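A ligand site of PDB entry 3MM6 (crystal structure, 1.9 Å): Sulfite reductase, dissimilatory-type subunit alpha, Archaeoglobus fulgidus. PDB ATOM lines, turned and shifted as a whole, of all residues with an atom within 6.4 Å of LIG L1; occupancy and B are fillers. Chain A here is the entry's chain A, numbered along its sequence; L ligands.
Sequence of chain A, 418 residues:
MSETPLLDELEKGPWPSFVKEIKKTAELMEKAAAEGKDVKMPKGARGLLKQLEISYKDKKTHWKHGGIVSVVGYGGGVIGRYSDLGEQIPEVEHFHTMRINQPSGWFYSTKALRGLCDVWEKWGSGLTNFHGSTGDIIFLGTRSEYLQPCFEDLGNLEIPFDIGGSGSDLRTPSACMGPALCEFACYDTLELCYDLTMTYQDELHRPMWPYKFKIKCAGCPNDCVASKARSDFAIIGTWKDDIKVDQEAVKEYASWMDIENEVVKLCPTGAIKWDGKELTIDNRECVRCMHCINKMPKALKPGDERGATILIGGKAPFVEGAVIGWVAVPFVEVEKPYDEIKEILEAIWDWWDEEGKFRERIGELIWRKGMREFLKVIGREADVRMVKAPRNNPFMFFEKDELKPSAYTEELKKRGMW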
ATOM      1  N   CYS A 176      -6.129 -21.572  -0.518  1.00  0.00           N
ATOM      2  CA  CYS A 176      -4.848 -22.291  -0.438  1.00  0.00           C
ATOM      3  C   CYS A 176      -5.097 -23.766  -0.048  1.00  0.00           C
ATOM      4  O   CYS A 176      -6.204 -24.120   0.315  1.00  0.00           O
ATOM      5  CB  CYS A 176      -3.984 -21.678   0.615  1.00  0.00           C
ATOM      6  SG  CYS A 176      -4.354 -22.121   2.335  1.00  0.00           S
ATOM      7  N   MET A 177      -4.053 -24.604  -0.125  1.00  0.00           N
ATOM      8  CA  MET A 177      -4.199 -26.055   0.107  1.00  0.00           C
ATOM      9  C   MET A 177      -4.695 -26.311   1.498  1.00  0.00           C
ATOM     10  O   MET A 177      -5.258 -27.366   1.764  1.00  0.00           O
ATOM     11  CB  MET A 177      -2.825 -26.770  -0.112  1.00  0.00           C
ATOM     12  CG  MET A 177      -1.733 -26.350   0.857  1.00  0.00           C
ATOM     13  SD  MET A 177      -0.128 -26.943   0.153  1.00  0.00           S
ATOM     14  CE  MET A 177       0.827 -26.412   1.565  1.00  0.00           C
ATOM     15  N   GLY A 178      -4.408 -25.395   2.417  1.00  0.00           N
ATOM     16  CA  GLY A 178      -4.917 -25.500   3.721  1.00  0.00           C
ATOM     17  C   GLY A 178      -4.643 -26.845   4.395  1.00  0.00           C
ATOM     18  O   GLY A 178      -3.545 -27.393   4.262  1.00  0.00           O
ATOM     19  N   PRO A 179      -5.644 -27.379   5.099  1.00  0.00           N
ATOM     20  CA  PRO A 179      -5.349 -28.536   5.941  1.00  0.00           C
ATOM     21  C   PRO A 179      -5.198 -29.800   5.098  1.00  0.00           C
ATOM     22  O   PRO A 179      -4.838 -30.808   5.669  1.00  0.00           O
ATOM     23  CB  PRO A 179      -6.561 -28.621   6.894  1.00  0.00           C
ATOM     24  CG  PRO A 179      -7.736 -27.958   6.014  1.00  0.00           C
ATOM     25  CD  PRO A 179      -7.021 -26.853   5.289  1.00  0.00           C
ATOM     26  N   CYS A 182      -1.159 -28.796   4.799  1.00  0.00           N
ATOM     27  CA  CYS A 182      -0.375 -27.834   5.522  1.00  0.00           C
ATOM     28  C   CYS A 182      -0.612 -27.866   7.025  1.00  0.00           C
ATOM     29  O   CYS A 182      -1.733 -27.781   7.474  1.00  0.00           O
ATOM     30  CB  CYS A 182      -0.616 -26.426   4.945  1.00  0.00           C
ATOM     31  SG  CYS A 182       0.489 -25.192   5.701  1.00  0.00           S
ATOM     32  N   GLU A 183       0.457 -27.923   7.820  1.00  0.00           N
ATOM     33  CA  GLU A 183       0.293 -28.039   9.237  1.00  0.00           C
ATOM     34  C   GLU A 183       0.071 -26.673   9.905  1.00  0.00           C
ATOM     35  O   GLU A 183      -0.117 -26.581  11.133  1.00  0.00           O
ATOM     36  CB  GLU A 183       1.526 -28.755   9.872  1.00  0.00           C
ATOM     37  CG  GLU A 183       2.838 -27.897   9.898  1.00  0.00           C
ATOM     38  CD  GLU A 183       3.647 -27.979   8.620  1.00  0.00           C
ATOM     39  OE1 GLU A 183       3.106 -28.291   7.499  1.00  0.00           O
ATOM     40  OE2 GLU A 183       4.852 -27.732   8.714  1.00  0.00           O
ATOM     41  N   PHE A 184       0.124 -25.600   9.124  1.00  0.00           N
ATOM     42  CA  PHE A 184      -0.106 -24.251   9.709  1.00  0.00           C
ATOM     43  C   PHE A 184      -1.603 -23.825   9.584  1.00  0.00           C
ATOM     44  O   PHE A 184      -2.022 -22.839  10.181  1.00  0.00           O
ATOM     45  CB  PHE A 184       0.730 -23.167   9.003  1.00  0.00           C
ATOM     46  CG  PHE A 184       2.244 -23.379   9.033  1.00  0.00           C
ATOM     47  CD1 PHE A 184       2.864 -24.218   9.950  1.00  0.00           C
ATOM     48  CD2 PHE A 184       3.048 -22.633   8.143  1.00  0.00           C
ATOM     49  CE1 PHE A 184       4.287 -24.332   9.957  1.00  0.00           C
ATOM     50  CE2 PHE A 184       4.401 -22.749   8.096  1.00  0.00           C
ATOM     51  CZ  PHE A 184       5.049 -23.591   8.997  1.00  0.00           C
ATOM     52  N   ALA A 185      -2.377 -24.534   8.779  1.00  0.00           N
ATOM     53  CA  ALA A 185      -3.768 -24.079   8.504  1.00  0.00           C
ATOM     54  C   ALA A 185      -4.624 -23.834   9.733  1.00  0.00           C
ATOM     55  O   ALA A 185      -4.707 -24.675  10.681  1.00  0.00           O
ATOM     56  CB  ALA A 185      -4.464 -25.055   7.531  1.00  0.00           C
ATOM     57  N   CYS A 186      -5.258 -22.684   9.762  1.00  0.00           N
ATOM     58  CA  CYS A 186      -6.077 -22.358  10.934  1.00  0.00           C
ATOM     59  C   CYS A 186      -7.588 -22.673  10.776  1.00  0.00           C
ATOM     60  O   CYS A 186      -8.301 -22.554  11.712  1.00  0.00           O
ATOM     61  CB  CYS A 186      -5.874 -20.892  11.344  1.00  0.00           C
ATOM     62  SG  CYS A 186      -4.259 -20.608  11.957  1.00  0.00           S
ATOM     63  N   THR A 189      -9.839 -24.340   4.686  1.00  0.00           N
ATOM     64  CA  THR A 189      -9.930 -23.389   3.571  1.00  0.00           C
ATOM     65  C   THR A 189     -10.735 -24.020   2.432  1.00  0.00           C
ATOM     66  O   THR A 189     -11.643 -23.369   1.874  1.00  0.00           O
ATOM     67  CB  THR A 189      -8.520 -22.945   3.106  1.00  0.00           C
ATOM     68  OG1 THR A 189      -7.769 -24.103   2.696  1.00  0.00           O
ATOM     69  CG2 THR A 189      -7.767 -22.190   4.256  1.00  0.00           C
ATOM     70  N   CYS A 217      -9.592 -17.510   0.207  1.00  0.00           N
ATOM     71  CA  CYS A 217      -9.449 -18.115   1.555  1.00  0.00           C
ATOM     72  C   CYS A 217      -8.033 -18.585   1.821  1.00  0.00           C
ATOM     73  O   CYS A 217      -7.593 -19.530   1.206  1.00  0.00           O
ATOM     74  CB  CYS A 217     -10.416 -19.332   1.670  1.00  0.00           C
ATOM     75  SG  CYS A 217     -12.137 -18.958   1.167  1.00  0.00           S
ATOM     76  N   ALA A 218      -7.348 -17.937   2.766  1.00  0.00           N
ATOM     77  CA  ALA A 218      -5.984 -18.332   3.155  1.00  0.00           C
ATOM     78  C   ALA A 218      -5.970 -18.958   4.535  1.00  0.00           C
ATOM     79  O   ALA A 218      -6.574 -18.387   5.460  1.00  0.00           O
ATOM     80  CB  ALA A 218      -5.025 -17.082   3.176  1.00  0.00           C
ATOM     81  N   GLY A 219      -5.153 -20.015   4.726  1.00  0.00           N
ATOM     82  CA  GLY A 219      -5.278 -20.823   5.962  1.00  0.00           C
ATOM     83  C   GLY A 219      -4.583 -20.144   7.101  1.00  0.00           C
ATOM     84  O   GLY A 219      -4.880 -20.458   8.251  1.00  0.00           O
ATOM     85  N   CYS A 220      -3.663 -19.222   6.803  1.00  0.00           N
ATOM     86  CA  CYS A 220      -2.929 -18.495   7.915  1.00  0.00           C
ATOM     87  C   CYS A 220      -2.349 -17.251   7.283  1.00  0.00           C
ATOM     88  O   CYS A 220      -2.448 -17.081   6.041  1.00  0.00           O
ATOM     89  CB  CYS A 220      -1.774 -19.356   8.466  1.00  0.00           C
ATOM     90  SG  CYS A 220      -0.362 -19.653   7.323  1.00  0.00           S
ATOM     91  N   PRO A 221      -1.719 -16.402   8.087  1.00  0.00           N
ATOM     92  CA  PRO A 221      -1.235 -15.126   7.674  1.00  0.00           C
ATOM     93  C   PRO A 221      -0.125 -15.146   6.618  1.00  0.00           C
ATOM     94  O   PRO A 221       0.149 -14.082   6.085  1.00  0.00           O
ATOM     95  CB  PRO A 221      -0.694 -14.501   8.965  1.00  0.00           C
ATOM     96  CG  PRO A 221      -1.429 -15.180  10.083  1.00  0.00           C
ATOM     97  CD  PRO A 221      -1.641 -16.581   9.554  1.00  0.00           C
ATOM     98  N   ASN A 222       0.474 -16.313   6.298  1.00  0.00           N
ATOM     99  CA  ASN A 222       1.364 -16.370   5.140  1.00  0.00           C
ATOM    100  C   ASN A 222       0.657 -15.963   3.846  1.00  0.00           C
ATOM    101  O   ASN A 222       1.310 -15.556   2.862  1.00  0.00           O
ATOM    102  CB  ASN A 222       2.034 -17.756   4.980  1.00  0.00           C
ATOM    103  CG  ASN A 222       3.109 -17.993   6.023  1.00  0.00           C
ATOM    104  OD1 ASN A 222       3.801 -17.076   6.462  1.00  0.00           O
ATOM    105  ND2 ASN A 222       3.216 -19.246   6.481  1.00  0.00           N
ATOM    106  N   ASP A 223      -0.669 -16.154   3.808  1.00  0.00           N
ATOM    107  CA  ASP A 223      -1.534 -15.818   2.666  1.00  0.00           C
ATOM    108  C   ASP A 223      -1.108 -16.378   1.338  1.00  0.00           C
ATOM    109  O   ASP A 223      -0.868 -15.621   0.389  1.00  0.00           O
ATOM    110  CB  ASP A 223      -1.588 -14.277   2.476  1.00  0.00           C
ATOM    111  CG  ASP A 223      -2.880 -13.797   1.805  1.00  0.00           C
ATOM    112  OD1 ASP A 223      -3.651 -14.609   1.204  1.00  0.00           O
ATOM    113  OD2 ASP A 223      -3.028 -12.553   1.731  1.00  0.00           O
ATOM    114  N   CYS A 224      -1.090 -17.693   1.200  1.00  0.00           N
ATOM    115  CA  CYS A 224      -0.488 -18.275  -0.016  1.00  0.00           C
ATOM    116  C   CYS A 224      -1.449 -18.273  -1.173  1.00  0.00           C
ATOM    117  O   CYS A 224      -1.174 -18.850  -2.240  1.00  0.00           O
ATOM    118  CB  CYS A 224      -0.035 -19.726   0.308  1.00  0.00           C
ATOM    119  SG  CYS A 224       1.139 -19.712   1.642  1.00  0.00           S
ATOM    120  N   VAL A 225      -2.611 -17.635  -1.007  1.00  0.00           N
ATOM    121  CA  VAL A 225      -3.426 -17.398  -2.268  1.00  0.00           C
ATOM    122  C   VAL A 225      -3.446 -15.897  -2.645  1.00  0.00           C
ATOM    123  O   VAL A 225      -4.169 -15.480  -3.513  1.00  0.00           O
ATOM    124  CB  VAL A 225      -4.894 -17.814  -2.186  1.00  0.00           C
ATOM    125  CG1 VAL A 225      -5.092 -19.203  -2.702  1.00  0.00           C
ATOM    126  CG2 VAL A 225      -5.463 -17.597  -0.832  1.00  0.00           C
ATOM    127  N   MET A 290       3.754 -15.104  11.696  1.00  0.00           N
ATOM    128  CA  MET A 290       4.114 -16.460  11.286  1.00  0.00           C
ATOM    129  C   MET A 290       5.637 -16.747  11.275  1.00  0.00           C
ATOM    130  O   MET A 290       6.033 -17.907  11.249  1.00  0.00           O
ATOM    131  CB  MET A 290       3.466 -16.881   9.947  1.00  0.00           C
ATOM    132  CG  MET A 290       1.932 -17.113  10.055  1.00  0.00           C
ATOM    133  SD  MET A 290       1.573 -18.536  11.131  1.00  0.00           S
ATOM    134  CE  MET A 290       2.176 -19.909  10.053  1.00  0.00           C
ATOM    135  N   ASN A 294       7.279 -20.327  10.898  1.00  0.00           N
ATOM    136  CA  ASN A 294       7.831 -20.693   9.566  1.00  0.00           C
ATOM    137  C   ASN A 294       9.260 -21.260   9.685  1.00  0.00           C
ATOM    138  O   ASN A 294       9.655 -22.156   8.909  1.00  0.00           O
ATOM    139  CB  ASN A 294       7.879 -19.499   8.595  1.00  0.00           C
ATOM    140  CG  ASN A 294       6.509 -18.960   8.205  1.00  0.00           C
ATOM    141  OD1 ASN A 294       5.512 -19.722   8.105  1.00  0.00           O
ATOM    142  ND2 ASN A 294       6.455 -17.634   7.893  1.00  0.00           N
HETATM  143 FE1  LIG L   1      -1.033 -20.800   5.589  1.00  0.00          FE
HETATM  144 FE2  LIG L   1       0.059 -21.115   3.204  1.00  0.00          FE
HETATM  145 FE3  LIG L   1      -0.382 -23.205   4.685  1.00  0.00          FE
HETATM  146 FE4  LIG L   1      -2.386 -21.919   3.577  1.00  0.00          FE
HETATM  147  S1  LIG L   1      -0.744 -23.058   2.498  1.00  0.00           S
HETATM  148  S2  LIG L   1      -2.296 -22.643   5.626  1.00  0.00           S
HETATM  149  S3  LIG L   1      -1.677 -19.852   3.721  1.00  0.00           S
HETATM  150  S4  LIG L   1       0.976 -21.539   5.146  1.00  0.00           S
HETATM  151 FE1  LG2 L   2       3.317 -20.416   0.685  1.00  0.00          FE
HETATM  152  C1  LG2 L   2       5.339 -21.220   3.320  1.00  0.00           C
HETATM  153  C2  LG2 L   2       2.842 -23.631   0.145  1.00  0.00           C
HETATM  154  C3  LG2 L   2       2.121 -19.659  -2.409  1.00  0.00           C
HETATM  155  C4  LG2 L   2       4.029 -17.148   1.124  1.00  0.00           C
HETATM  156  N1  LG2 L   2       3.754 -22.089   1.656  1.00  0.00           N
HETATM  157  C5  LG2 L   2       4.575 -22.239   2.745  1.00  0.00           C
HETATM  158  C6  LG2 L   2       4.714 -23.633   3.315  1.00  0.00           C
HETATM  159  C7  LG2 L   2       6.158 -24.001   3.799  1.00  0.00           C
HETATM  160  C8  LG2 L   2       3.740 -23.904   4.486  1.00  0.00           C
HETATM  161  C9  LG2 L   2       3.810 -25.379   4.965  1.00  0.00           C
HETATM  162  O1  LG2 L   2       3.824 -26.385   4.205  1.00  0.00           O
HETATM  163  O2  LG2 L   2       3.831 -25.494   6.182  1.00  0.00           O
HETATM  164  C10 LG2 L   2       4.291 -24.410   2.085  1.00  0.00           C
HETATM  165  C11 LG2 L   2       5.526 -24.958   1.265  1.00  0.00           C
HETATM  166  C12 LG2 L   2       6.254 -23.832   0.406  1.00  0.00           C
HETATM  167  C13 LG2 L   2       7.725 -24.062   0.124  1.00  0.00           C
HETATM  168  O3  LG2 L   2       8.087 -24.278  -1.049  1.00  0.00           O
HETATM  169  O4  LG2 L   2       8.540 -23.976   1.086  1.00  0.00           O
HETATM  170  C14 LG2 L   2       3.620 -23.310   1.262  1.00  0.00           C
HETATM  171  N2  LG2 L   2       2.650 -21.466  -0.787  1.00  0.00           N
HETATM  172  C15 LG2 L   2       2.420 -22.768  -0.801  1.00  0.00           C
HETATM  173  C16 LG2 L   2       1.659 -23.336  -2.048  1.00  0.00           C
HETATM  174  C17 LG2 L   2       1.876 -24.766  -2.523  1.00  0.00           C
HETATM  175  C18 LG2 L   2       0.148 -23.094  -1.716  1.00  0.00           C
HETATM  176  C19 LG2 L   2      -0.939 -23.603  -2.669  1.00  0.00           C
HETATM  177  O5  LG2 L   2      -2.083 -23.817  -2.251  1.00  0.00           O
HETATM  178  O6  LG2 L   2      -0.727 -23.835  -3.879  1.00  0.00           O
HETATM  179  C20 LG2 L   2       1.978 -22.134  -2.853  1.00  0.00           C
HETATM  180  C21 LG2 L   2       2.895 -22.440  -4.048  1.00  0.00           C
HETATM  181  C22 LG2 L   2       3.343 -21.326  -5.045  1.00  0.00           C
HETATM  182  C23 LG2 L   2       4.430 -21.884  -5.918  1.00  0.00           C
HETATM  183  O7  LG2 L   2       4.255 -22.827  -6.765  1.00  0.00           O
HETATM  184  O8  LG2 L   2       5.558 -21.338  -5.781  1.00  0.00           O
HETATM  185  C24 LG2 L   2       2.249 -20.954  -2.015  1.00  0.00           C
HETATM  186  N3  LG2 L   2       3.212 -18.755  -0.432  1.00  0.00           N
HETATM  187  C25 LG2 L   2       2.548 -18.648  -1.593  1.00  0.00           C
HETATM  188  C26 LG2 L   2       2.380 -17.254  -2.072  1.00  0.00           C
HETATM  189  C27 LG2 L   2       1.258 -16.711  -2.929  1.00  0.00           C
HETATM  190  C28 LG2 L   2       1.905 -16.097  -4.213  1.00  0.00           C
HETATM  191  O9  LG2 L   2       3.141 -15.954  -4.386  1.00  0.00           O
HETATM  192  O10 LG2 L   2       1.112 -15.666  -5.072  1.00  0.00           O
HETATM  193  C29 LG2 L   2       3.033 -16.438  -1.017  1.00  0.00           C
HETATM  194  C30 LG2 L   2       2.658 -15.000  -0.651  1.00  0.00           C
HETATM  195  C31 LG2 L   2       3.863 -14.301  -1.361  1.00  0.00           C
HETATM  196  C32 LG2 L   2       4.307 -13.011  -0.715  1.00  0.00           C
HETATM  197  O11 LG2 L   2       4.447 -11.992  -1.426  1.00  0.00           O
HETATM  198  O12 LG2 L   2       4.548 -12.944   0.518  1.00  0.00           O
HETATM  199  C33 LG2 L   2       3.438 -17.550  -0.051  1.00  0.00           C
HETATM  200  N4  LG2 L   2       4.307 -19.380   1.991  1.00  0.00           N
HETATM  201  C34 LG2 L   2       4.541 -18.031   2.023  1.00  0.00           C
HETATM  202  C35 LG2 L   2       5.364 -17.514   3.215  1.00  0.00           C
HETATM  203  C36 LG2 L   2       6.162 -16.195   3.317  1.00  0.00           C
HETATM  204  C37 LG2 L   2       7.634 -16.138   2.960  1.00  0.00           C
HETATM  205  C38 LG2 L   2       8.244 -14.864   3.551  1.00  0.00           C
HETATM  206  O13 LG2 L   2       9.417 -15.001   3.904  1.00  0.00           O
HETATM  207  O14 LG2 L   2       7.629 -13.748   3.620  1.00  0.00           O
HETATM  208  C39 LG2 L   2       5.788 -18.838   3.827  1.00  0.00           C
HETATM  209  C40 LG2 L   2       6.813 -19.090   4.927  1.00  0.00           C
HETATM  210  C41 LG2 L   2       8.061 -19.848   4.526  1.00  0.00           C
HETATM  211  O15 LG2 L   2       8.848 -19.351   3.682  1.00  0.00           O
HETATM  212  O16 LG2 L   2       8.245 -20.981   5.071  1.00  0.00           O
HETATM  213  C42 LG2 L   2       5.177 -19.894   2.927  1.00  0.00           C
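N of Cys 220 sits close to S3 of LIG L1.
An iron atom (FE1) of LIG L1 is bound by the side-chain sulfur of Cys 220 (2.2 Å).
FE4 of LIG L1 is bound by SG of Cys 176 (2.3 Å).
The backbone NH (N) of Cys 224 sits close to a sulfur (S3) of LIG L1.
The side-chain sulfur (SG) of Cys 224 is bound to an iron atom (FE2) of LIG L1.
An iron atom (FE3) of LIG L1 is bound by the side-chain sulfur (SG) of Cys 182 (2.4 Å).
ND2 of Asn 222 lies close to S4 of LIG L1 (3.5 Å).
A sulfur (S3) of LIG L1 lies close to the backbone NH of Gly 219, at 3.6 Å.
A sulfur (S2) of LIG L1 lies close to the backbone NH (N) of Ala 185 (3.7 Å).
An iron atom (FE1) of LG2 L2 is bound by the side-chain sulfur (SG) of Cys 224.
The side-chain sulfur of Cys 182 lies close to an oxygen (O2) of LG2 L2 (3.4 Å).
O5 of LG2 L2 sits at hydrogen-bond distance from N of Met 177 (3.0 Å).
N of Asn 222 lies close to SG of Cys 220, 3.6 Å away.
N of Gly 219 sits close to SG of Cys 176.
The backbone NH (N) of Gly 178 sits close to the side-chain sulfur (SG) of Cys 176, at 3.3 Å.
The backbone carbonyl oxygen of Cys 176 is in hydrogen-bond range of the side-chain hydroxyl of Thr 189, 2.8 Å away.
The backbone NH (N) of Cys 176 lies within hydrogen-bond range of the backbone carbonyl oxygen (O) of Cys 217 (3.0 Å).
N of Phe 184 lies close to SG of Cys 182 (3.5 Å).
The side-chain amide nitrogen of Asn 222 sits at hydrogen-bond distance from the side-chain amide oxygen of Asn 294, 2.9 Å away.
The backbone carbonyl oxygen (O) of Phe 184 sits at hydrogen-bond distance from the side-chain sulfur (SG) of Cys 186, 3.6 Å away.
Met 177 touches LIG L1.
Phe 184 touches LIG L1 (CD2 to S4, 3.8 Å).
N of Asp 223 touches S3 of LIG L1 (3.8 Å).
Hydrophobic or aromatic side chains that line LIG L1: Met 177, Phe 184 and Ala 185.
Ten residues have an atom within 4 Å of LIG L1: Cys 176, Met 177, Cys 182, Phe 184, Ala 185, Gly 219, Cys 220, Asn 222, Asp 223 and Cys 224.
The nearest printed residue that does not touch LIG L1 is Gly 178 (4.2 Å).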
